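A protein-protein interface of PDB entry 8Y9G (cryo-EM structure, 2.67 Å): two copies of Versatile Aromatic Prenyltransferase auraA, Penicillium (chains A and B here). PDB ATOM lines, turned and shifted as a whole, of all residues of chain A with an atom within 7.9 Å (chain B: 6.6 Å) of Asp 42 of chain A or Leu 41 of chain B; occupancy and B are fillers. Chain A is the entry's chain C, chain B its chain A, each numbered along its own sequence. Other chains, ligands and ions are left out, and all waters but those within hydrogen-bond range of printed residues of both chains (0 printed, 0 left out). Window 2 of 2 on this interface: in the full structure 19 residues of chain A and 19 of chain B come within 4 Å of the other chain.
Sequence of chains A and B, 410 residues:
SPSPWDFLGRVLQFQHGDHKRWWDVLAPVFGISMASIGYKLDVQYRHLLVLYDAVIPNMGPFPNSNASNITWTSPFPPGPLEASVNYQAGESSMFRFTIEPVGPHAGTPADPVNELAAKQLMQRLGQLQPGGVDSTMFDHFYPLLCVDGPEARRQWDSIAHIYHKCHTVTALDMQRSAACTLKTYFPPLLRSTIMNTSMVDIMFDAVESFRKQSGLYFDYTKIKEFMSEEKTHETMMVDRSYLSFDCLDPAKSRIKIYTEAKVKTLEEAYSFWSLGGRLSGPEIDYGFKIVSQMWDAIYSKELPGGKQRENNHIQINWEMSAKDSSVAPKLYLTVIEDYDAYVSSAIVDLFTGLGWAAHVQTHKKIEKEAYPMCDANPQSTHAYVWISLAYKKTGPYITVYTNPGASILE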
ATOM      1  N   PRO A   4     -22.331 -26.944 -10.019  1.00  0.00           N
ATOM      2  CA  PRO A   4     -21.115 -26.761  -9.212  1.00  0.00           C
ATOM      3  C   PRO A   4     -21.283 -27.079  -7.736  1.00  0.00           C
ATOM      4  O   PRO A   4     -20.359 -27.626  -7.126  1.00  0.00           O
ATOM      5  CB  PRO A   4     -20.780 -25.285  -9.444  1.00  0.00           C
ATOM      6  CG  PRO A   4     -21.314 -24.992 -10.778  1.00  0.00           C
ATOM      7  CD  PRO A   4     -22.540 -25.825 -10.953  1.00  0.00           C
ATOM      8  N   TYR A  39     -23.906 -16.088 -14.273  1.00  0.00           N
ATOM      9  CA  TYR A  39     -22.508 -16.274 -13.932  1.00  0.00           C
ATOM     10  C   TYR A  39     -21.969 -17.525 -14.611  1.00  0.00           C
ATOM     11  O   TYR A  39     -22.679 -18.509 -14.823  1.00  0.00           O
ATOM     12  CB  TYR A  39     -22.328 -16.386 -12.422  1.00  0.00           C
ATOM     13  CG  TYR A  39     -22.439 -15.084 -11.668  1.00  0.00           C
ATOM     14  CD1 TYR A  39     -23.133 -14.010 -12.191  1.00  0.00           C
ATOM     15  CD2 TYR A  39     -21.856 -14.937 -10.421  1.00  0.00           C
ATOM     16  CE1 TYR A  39     -23.241 -12.831 -11.501  1.00  0.00           C
ATOM     17  CE2 TYR A  39     -21.962 -13.761  -9.724  1.00  0.00           C
ATOM     18  CZ  TYR A  39     -22.654 -12.712 -10.267  1.00  0.00           C
ATOM     19  OH  TYR A  39     -22.750 -11.541  -9.563  1.00  0.00           O
ATOM     20  N   LYS A  40     -20.691 -17.475 -14.956  1.00  0.00           N
ATOM     21  CA  LYS A  40     -20.044 -18.577 -15.643  1.00  0.00           C
ATOM     22  C   LYS A  40     -19.604 -19.641 -14.648  1.00  0.00           C
ATOM     23  O   LYS A  40     -19.293 -19.358 -13.490  1.00  0.00           O
ATOM     24  CB  LYS A  40     -18.856 -18.068 -16.454  1.00  0.00           C
ATOM     25  CG  LYS A  40     -19.262 -17.123 -17.559  1.00  0.00           C
ATOM     26  CD  LYS A  40     -18.151 -16.899 -18.561  1.00  0.00           C
ATOM     27  CE  LYS A  40     -17.176 -15.856 -18.072  1.00  0.00           C
ATOM     28  NZ  LYS A  40     -17.523 -14.507 -18.579  1.00  0.00           N
ATOM     29  N   LEU A  41     -19.588 -20.887 -15.121  1.00  0.00           N
ATOM     30  CA  LEU A  41     -19.357 -22.020 -14.233  1.00  0.00           C
ATOM     31  C   LEU A  41     -18.070 -21.857 -13.436  1.00  0.00           C
ATOM     32  O   LEU A  41     -18.021 -22.204 -12.253  1.00  0.00           O
ATOM     33  CB  LEU A  41     -19.335 -23.311 -15.042  1.00  0.00           C
ATOM     34  CG  LEU A  41     -20.639 -23.655 -15.753  1.00  0.00           C
ATOM     35  CD1 LEU A  41     -20.413 -24.685 -16.829  1.00  0.00           C
ATOM     36  CD2 LEU A  41     -21.632 -24.166 -14.752  1.00  0.00           C
ATOM     37  N   ASP A  42     -17.017 -21.332 -14.063  1.00  0.00           N
ATOM     38  CA  ASP A  42     -15.790 -21.070 -13.321  1.00  0.00           C
ATOM     39  C   ASP A  42     -16.015 -20.020 -12.243  1.00  0.00           C
ATOM     40  O   ASP A  42     -15.457 -20.117 -11.143  1.00  0.00           O
ATOM     41  CB  ASP A  42     -14.683 -20.634 -14.277  1.00  0.00           C
ATOM     42  CG  ASP A  42     -15.068 -19.441 -15.116  1.00  0.00           C
ATOM     43  OD1 ASP A  42     -15.973 -19.582 -15.962  1.00  0.00           O
ATOM     44  OD2 ASP A  42     -14.459 -18.368 -14.939  1.00  0.00           O
ATOM     45  N   VAL A  43     -16.849 -19.020 -12.532  1.00  0.00           N
ATOM     46  CA  VAL A  43     -17.141 -17.985 -11.548  1.00  0.00           C
ATOM     47  C   VAL A  43     -17.958 -18.562 -10.402  1.00  0.00           C
ATOM     48  O   VAL A  43     -17.716 -18.252  -9.232  1.00  0.00           O
ATOM     49  CB  VAL A  43     -17.856 -16.803 -12.221  1.00  0.00           C
ATOM     50  CG1 VAL A  43     -18.226 -15.764 -11.207  1.00  0.00           C
ATOM     51  CG2 VAL A  43     -16.984 -16.197 -13.283  1.00  0.00           C
ATOM     52  N   GLN A  44     -18.950 -19.395 -10.720  1.00  0.00           N
ATOM     53  CA  GLN A  44     -19.689 -20.093  -9.675  1.00  0.00           C
ATOM     54  C   GLN A  44     -18.759 -20.917  -8.799  1.00  0.00           C
ATOM     55  O   GLN A  44     -18.884 -20.907  -7.572  1.00  0.00           O
ATOM     56  CB  GLN A  44     -20.755 -20.993 -10.287  1.00  0.00           C
ATOM     57  CG  GLN A  44     -21.792 -20.283 -11.110  1.00  0.00           C
ATOM     58  CD  GLN A  44     -22.800 -21.234 -11.699  1.00  0.00           C
ATOM     59  OE1 GLN A  44     -23.225 -22.187 -11.050  1.00  0.00           O
ATOM     60  NE2 GLN A  44     -23.186 -20.987 -12.937  1.00  0.00           N
ATOM     61  N   TYR A  45     -17.839 -21.657  -9.414  1.00  0.00           N
ATOM     62  CA  TYR A  45     -16.890 -22.457  -8.648  1.00  0.00           C
ATOM     63  C   TYR A  45     -16.063 -21.580  -7.719  1.00  0.00           C
ATOM     64  O   TYR A  45     -15.930 -21.872  -6.526  1.00  0.00           O
ATOM     65  CB  TYR A  45     -15.987 -23.238  -9.600  1.00  0.00           C
ATOM     66  CG  TYR A  45     -16.510 -24.602  -9.975  1.00  0.00           C
ATOM     67  CD1 TYR A  45     -16.440 -25.660  -9.086  1.00  0.00           C
ATOM     68  CD2 TYR A  45     -17.068 -24.834 -11.219  1.00  0.00           C
ATOM     69  CE1 TYR A  45     -16.917 -26.903  -9.424  1.00  0.00           C
ATOM     70  CE2 TYR A  45     -17.547 -26.071 -11.565  1.00  0.00           C
ATOM     71  CZ  TYR A  45     -17.468 -27.104 -10.664  1.00  0.00           C
ATOM     72  OH  TYR A  45     -17.946 -28.345 -10.996  1.00  0.00           O
ATOM     73  N   ARG A  46     -15.497 -20.496  -8.251  1.00  0.00           N
ATOM     74  CA  ARG A  46     -14.679 -19.607  -7.435  1.00  0.00           C
ATOM     75  C   ARG A  46     -15.477 -19.016  -6.281  1.00  0.00           C
ATOM     76  O   ARG A  46     -14.999 -18.972  -5.143  1.00  0.00           O
ATOM     77  CB  ARG A  46     -14.097 -18.498  -8.305  1.00  0.00           C
ATOM     78  CG  ARG A  46     -13.052 -18.977  -9.281  1.00  0.00           C
ATOM     79  CD  ARG A  46     -12.412 -17.832 -10.033  1.00  0.00           C
ATOM     80  NE  ARG A  46     -11.785 -16.877  -9.128  1.00  0.00           N
ATOM     81  CZ  ARG A  46     -11.085 -15.823  -9.527  1.00  0.00           C
ATOM     82  NH1 ARG A  46     -10.913 -15.588 -10.820  1.00  0.00           N
ATOM     83  NH2 ARG A  46     -10.554 -15.006  -8.631  1.00  0.00           N
ATOM     84  N   HIS A  47     -16.701 -18.565  -6.550  1.00  0.00           N
ATOM     85  CA  HIS A  47     -17.483 -17.895  -5.519  1.00  0.00           C
ATOM     86  C   HIS A  47     -17.976 -18.875  -4.466  1.00  0.00           C
ATOM     87  O   HIS A  47     -18.022 -18.544  -3.277  1.00  0.00           O
ATOM     88  CB  HIS A  47     -18.649 -17.156  -6.161  1.00  0.00           C
ATOM     89  CG  HIS A  47     -18.260 -15.867  -6.804  1.00  0.00           C
ATOM     90  ND1 HIS A  47     -17.215 -15.097  -6.344  1.00  0.00           N
ATOM     91  CD2 HIS A  47     -18.766 -15.214  -7.875  1.00  0.00           C
ATOM     92  CE1 HIS A  47     -17.098 -14.023  -7.100  1.00  0.00           C
ATOM     93  NE2 HIS A  47     -18.027 -14.070  -8.036  1.00  0.00           N
ATOM     94  N   LEU A  48     -18.347 -20.085  -4.875  1.00  0.00           N
ATOM     95  CA  LEU A  48     -18.736 -21.096  -3.907  1.00  0.00           C
ATOM     96  C   LEU A  48     -17.547 -21.572  -3.091  1.00  0.00           C
ATOM     97  O   LEU A  48     -17.700 -21.901  -1.914  1.00  0.00           O
ATOM     98  CB  LEU A  48     -19.402 -22.263  -4.624  1.00  0.00           C
ATOM     99  CG  LEU A  48     -20.784 -21.970  -5.201  1.00  0.00           C
ATOM    100  CD1 LEU A  48     -21.124 -22.943  -6.295  1.00  0.00           C
ATOM    101  CD2 LEU A  48     -21.826 -22.012  -4.109  1.00  0.00           C
ATOM    102  N   LEU A  49     -16.350 -21.571  -3.672  1.00  0.00           N
ATOM    103  CA  LEU A  49     -15.162 -21.914  -2.900  1.00  0.00           C
ATOM    104  C   LEU A  49     -14.807 -20.804  -1.919  1.00  0.00           C
ATOM    105  O   LEU A  49     -14.305 -21.071  -0.823  1.00  0.00           O
ATOM    106  CB  LEU A  49     -14.001 -22.198  -3.846  1.00  0.00           C
ATOM    107  CG  LEU A  49     -14.149 -23.465  -4.683  1.00  0.00           C
ATOM    108  CD1 LEU A  49     -13.333 -23.386  -5.958  1.00  0.00           C
ATOM    109  CD2 LEU A  49     -13.759 -24.668  -3.875  1.00  0.00           C
ATOM    110  N   ARG A 176     -19.482 -10.769 -11.379  1.00  0.00           N
ATOM    111  CA  ARG A 176     -19.412 -11.686 -12.504  1.00  0.00           C
ATOM    112  C   ARG A 176     -17.979 -11.985 -12.916  1.00  0.00           C
ATOM    113  O   ARG A 176     -17.743 -12.958 -13.639  1.00  0.00           O
ATOM    114  CB  ARG A 176     -20.187 -11.085 -13.673  1.00  0.00           C
ATOM    115  CG  ARG A 176     -20.872 -12.075 -14.567  1.00  0.00           C
ATOM    116  CD  ARG A 176     -21.696 -11.337 -15.598  1.00  0.00           C
ATOM    117  NE  ARG A 176     -22.885 -10.740 -14.996  1.00  0.00           N
ATOM    118  CZ  ARG A 176     -24.130 -11.162 -15.184  1.00  0.00           C
ATOM    119  NH1 ARG A 176     -24.399 -12.189 -15.977  1.00  0.00           N
ATOM    120  NH2 ARG A 176     -25.124 -10.538 -14.581  1.00  0.00           N
ATOM    121  N   SER A 177     -17.022 -11.175 -12.469  1.00  0.00           N
ATOM    122  CA  SER A 177     -15.615 -11.329 -12.800  1.00  0.00           C
ATOM    123  C   SER A 177     -14.867 -12.195 -11.797  1.00  0.00           C
ATOM    124  O   SER A 177     -13.635 -12.247 -11.836  1.00  0.00           O
ATOM    125  CB  SER A 177     -14.956  -9.956 -12.882  1.00  0.00           C
ATOM    126  OG  SER A 177     -14.973  -9.316 -11.617  1.00  0.00           O
ATOM    127  N   ALA A 178     -15.580 -12.865 -10.900  1.00  0.00           N
ATOM    128  CA  ALA A 178     -15.036 -13.714  -9.848  1.00  0.00           C
ATOM    129  C   ALA A 178     -14.362 -12.904  -8.751  1.00  0.00           C
ATOM    130  O   ALA A 178     -13.803 -13.495  -7.816  1.00  0.00           O
ATOM    131  CB  ALA A 178     -14.040 -14.737 -10.388  1.00  0.00           C
ATOM    132  N   PRO B   2      -6.315 -15.703 -11.038  1.00  0.00           N
ATOM    133  CA  PRO B   2      -5.539 -16.896 -10.696  1.00  0.00           C
ATOM    134  C   PRO B   2      -5.969 -18.103 -11.509  1.00  0.00           C
ATOM    135  O   PRO B   2      -7.120 -18.225 -11.934  1.00  0.00           O
ATOM    136  CB  PRO B   2      -5.835 -17.101  -9.206  1.00  0.00           C
ATOM    137  CG  PRO B   2      -7.131 -16.440  -8.990  1.00  0.00           C
ATOM    138  CD  PRO B   2      -7.155 -15.264  -9.913  1.00  0.00           C
ATOM    139  N   SER B   3      -5.016 -19.000 -11.726  1.00  0.00           N
ATOM    140  CA  SER B   3      -5.313 -20.247 -12.400  1.00  0.00           C
ATOM    141  C   SER B   3      -6.000 -21.210 -11.435  1.00  0.00           C
ATOM    142  O   SER B   3      -5.783 -21.145 -10.223  1.00  0.00           O
ATOM    143  CB  SER B   3      -4.039 -20.869 -12.944  1.00  0.00           C
ATOM    144  OG  SER B   3      -3.235 -21.361 -11.890  1.00  0.00           O
ATOM    145  N   PRO B   4      -6.833 -22.116 -11.947  1.00  0.00           N
ATOM    146  CA  PRO B   4      -7.630 -22.964 -11.047  1.00  0.00           C
ATOM    147  C   PRO B   4      -6.830 -23.646  -9.952  1.00  0.00           C
ATOM    148  O   PRO B   4      -7.329 -23.775  -8.829  1.00  0.00           O
ATOM    149  CB  PRO B   4      -8.258 -23.974 -12.009  1.00  0.00           C
ATOM    150  CG  PRO B   4      -8.365 -23.252 -13.283  1.00  0.00           C
ATOM    151  CD  PRO B   4      -7.201 -22.323 -13.359  1.00  0.00           C
ATOM    152  N   GLY B  38      -6.740 -27.102 -23.985  1.00  0.00           N
ATOM    153  CA  GLY B  38      -7.859 -26.233 -24.271  1.00  0.00           C
ATOM    154  C   GLY B  38      -9.066 -26.550 -23.419  1.00  0.00           C
ATOM    155  O   GLY B  38     -10.187 -26.152 -23.746  1.00  0.00           O
ATOM    156  N   TYR B  39      -8.854 -27.276 -22.326  1.00  0.00           N
ATOM    157  CA  TYR B  39      -9.945 -27.577 -21.419  1.00  0.00           C
ATOM    158  C   TYR B  39     -10.509 -26.287 -20.838  1.00  0.00           C
ATOM    159  O   TYR B  39      -9.799 -25.301 -20.631  1.00  0.00           O
ATOM    160  CB  TYR B  39      -9.477 -28.491 -20.291  1.00  0.00           C
ATOM    161  CG  TYR B  39      -9.276 -29.935 -20.682  1.00  0.00           C
ATOM    162  CD1 TYR B  39      -9.033 -30.295 -21.994  1.00  0.00           C
ATOM    163  CD2 TYR B  39      -9.319 -30.939 -19.729  1.00  0.00           C
ATOM    164  CE1 TYR B  39      -8.842 -31.605 -22.346  1.00  0.00           C
ATOM    165  CE2 TYR B  39      -9.127 -32.252 -20.075  1.00  0.00           C
ATOM    166  CZ  TYR B  39      -8.889 -32.580 -21.382  1.00  0.00           C
ATOM    167  OH  TYR B  39      -8.702 -33.894 -21.716  1.00  0.00           O
ATOM    168  N   LYS B  40     -11.806 -26.305 -20.576  1.00  0.00           N
ATOM    169  CA  LYS B  40     -12.493 -25.139 -20.053  1.00  0.00           C
ATOM    170  C   LYS B  40     -12.318 -25.050 -18.542  1.00  0.00           C
ATOM    171  O   LYS B  40     -12.174 -26.055 -17.846  1.00  0.00           O
ATOM    172  CB  LYS B  40     -13.973 -25.188 -20.425  1.00  0.00           C
ATOM    173  CG  LYS B  40     -14.204 -25.122 -21.916  1.00  0.00           C
ATOM    174  CD  LYS B  40     -15.645 -24.822 -22.259  1.00  0.00           C
ATOM    175  CE  LYS B  40     -16.490 -26.073 -22.217  1.00  0.00           C
ATOM    176  NZ  LYS B  40     -16.597 -26.703 -23.554  1.00  0.00           N
ATOM    177  N   LEU B  41     -12.328 -23.814 -18.044  1.00  0.00           N
ATOM    178  CA  LEU B  41     -11.997 -23.572 -16.644  1.00  0.00           C
ATOM    179  C   LEU B  41     -12.859 -24.408 -15.710  1.00  0.00           C
ATOM    180  O   LEU B  41     -12.368 -24.916 -14.697  1.00  0.00           O
ATOM    181  CB  LEU B  41     -12.141 -22.087 -16.334  1.00  0.00           C
ATOM    182  CG  LEU B  41     -11.201 -21.167 -17.104  1.00  0.00           C
ATOM    183  CD1 LEU B  41     -11.678 -19.738 -17.050  1.00  0.00           C
ATOM    184  CD2 LEU B  41      -9.820 -21.269 -16.526  1.00  0.00           C
ATOM    185  N   ASP B  42     -14.143 -24.566 -16.028  1.00  0.00           N
ATOM    186  CA  ASP B  42     -14.989 -25.433 -15.215  1.00  0.00           C
ATOM    187  C   ASP B  42     -14.515 -26.877 -15.281  1.00  0.00           C
ATOM    188  O   ASP B  42     -14.556 -27.598 -14.277  1.00  0.00           O
ATOM    189  CB  ASP B  42     -16.442 -25.320 -15.668  1.00  0.00           C
ATOM    190  CG  ASP B  42     -16.624 -25.615 -17.137  1.00  0.00           C
ATOM    191  OD1 ASP B  42     -16.130 -24.823 -17.964  1.00  0.00           O
ATOM    192  OD2 ASP B  42     -17.270 -26.631 -17.465  1.00  0.00           O
ATOM    193  N   VAL B  43     -14.039 -27.309 -16.449  1.00  0.00           N
ATOM    194  CA  VAL B  43     -13.540 -28.672 -16.592  1.00  0.00           C
ATOM    195  C   VAL B  43     -12.249 -28.847 -15.808  1.00  0.00           C
ATOM    196  O   VAL B  43     -12.041 -29.870 -15.148  1.00  0.00           O
ATOM    197  CB  VAL B  43     -13.356 -29.013 -18.079  1.00  0.00           C
ATOM    198  CG1 VAL B  43     -12.775 -30.385 -18.237  1.00  0.00           C
ATOM    199  CG2 VAL B  43     -14.667 -28.924 -18.805  1.00  0.00           C
ATOM    200  N   GLN B  44     -11.353 -27.862 -15.881  1.00  0.00           N
ATOM    201  CA  GLN B  44     -10.154 -27.892 -15.053  1.00  0.00           C
ATOM    202  C   GLN B  44     -10.506 -27.983 -13.578  1.00  0.00           C
ATOM    203  O   GLN B  44      -9.898 -28.759 -12.836  1.00  0.00           O
ATOM    204  CB  GLN B  44      -9.300 -26.656 -15.306  1.00  0.00           C
ATOM    205  CG  GLN B  44      -8.813 -26.496 -16.718  1.00  0.00           C
ATOM    206  CD  GLN B  44      -7.993 -25.245 -16.898  1.00  0.00           C
ATOM    207  OE1 GLN B  44      -7.197 -24.880 -16.037  1.00  0.00           O
ATOM    208  NE2 GLN B  44      -8.186 -24.575 -18.019  1.00  0.00           N
ATOM    209  N   TYR B  45     -11.466 -27.179 -13.129  1.00  0.00           N
ATOM    210  CA  TYR B  45     -11.883 -27.222 -11.732  1.00  0.00           C
ATOM    211  C   TYR B  45     -12.390 -28.606 -11.354  1.00  0.00           C
ATOM    212  O   TYR B  45     -11.980 -29.173 -10.338  1.00  0.00           O
ATOM    213  CB  TYR B  45     -12.961 -26.166 -11.484  1.00  0.00           C
ATOM    214  CG  TYR B  45     -12.426 -24.819 -11.062  1.00  0.00           C
ATOM    215  CD1 TYR B  45     -11.961 -24.608  -9.777  1.00  0.00           C
ATOM    216  CD2 TYR B  45     -12.391 -23.758 -11.950  1.00  0.00           C
ATOM    217  CE1 TYR B  45     -11.472 -23.383  -9.392  1.00  0.00           C
ATOM    218  CE2 TYR B  45     -11.905 -22.532 -11.573  1.00  0.00           C
ATOM    219  CZ  TYR B  45     -11.447 -22.350 -10.292  1.00  0.00           C
ATOM    220  OH  TYR B  45     -10.957 -21.129  -9.904  1.00  0.00           O
ATOM    221  N   ARG B  46     -13.287 -29.166 -12.169  1.00  0.00           N
ATOM    222  CA  ARG B  46     -13.833 -30.487 -11.877  1.00  0.00           C
ATOM    223  C   ARG B  46     -12.740 -31.546 -11.830  1.00  0.00           C
ATOM    224  O   ARG B  46     -12.715 -32.385 -10.924  1.00  0.00           O
ATOM    225  CB  ARG B  46     -14.885 -30.851 -12.920  1.00  0.00           C
ATOM    226  CG  ARG B  46     -16.145 -30.029 -12.822  1.00  0.00           C
ATOM    227  CD  ARG B  46     -17.206 -30.508 -13.787  1.00  0.00           C
ATOM    228  NE  ARG B  46     -17.556 -31.903 -13.558  1.00  0.00           N
ATOM    229  CZ  ARG B  46     -18.515 -32.548 -14.211  1.00  0.00           C
ATOM    230  NH1 ARG B  46     -19.231 -31.920 -15.133  1.00  0.00           N
ATOM    231  NH2 ARG B  46     -18.757 -33.820 -13.939  1.00  0.00           N
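Hydrophobic or aromatic side chains of chain A within 4 Å of the printed part of chain B: Leu 41, Tyr 45 and Leu 49.
Along chain A the printed residues that touch a printed residue of chain B span positions 41 to 49.
Hydrophobic or aromatic side chains of chain B that line the printed part of chain A: Pro 2, Leu 41 and Tyr 45.
Among the printed residues, 6 pairs touch across the chains.
Leu 41 of chain A touches Asp 42 of chain B, and with the chains exchanged Asp 42 of chain A touches Leu 41 of chain B.
Tyr 45 of chain A touches Arg 46 of chain B, and with the chains exchanged Arg 46 of chain A touches Tyr 45 of chain B.
Among the printed residues, merely in contact across the chains: Arg 46 of chain A with Tyr 45 of chain B (3.1 Å), Tyr 45 of chain A with Arg 46 of chain B (3.1 Å), Leu 41 of chain A with Asp 42 of chain B (3.6 Å), Asp 42 of chain A with Leu 41 of chain B (3.6 Å), Arg 46 of chain A with Pro 2 of chain B (3.6 Å) and Leu 49 of chain A with Tyr 45 of chain B (3.9 Å).
Of chain B, only Leu 41 (3.6 Å) comes within 4 Å of Asp 42 of chain A.
Leu 41 of chain B touches one residue of chain A.
Of the printed residues of chain A, Arg 46 of chain B touches Tyr 45 (3.1 Å).
Printed residues of chain A within 4 Å of Tyr 45 of chain B: Arg 46 (3.1 Å) and Leu 49 (3.9 Å).
Of the printed residues of chain B, Leu 49 of chain A touches Tyr 45.
Tyr 39 of chain A touches none of the printed residues of chain B.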
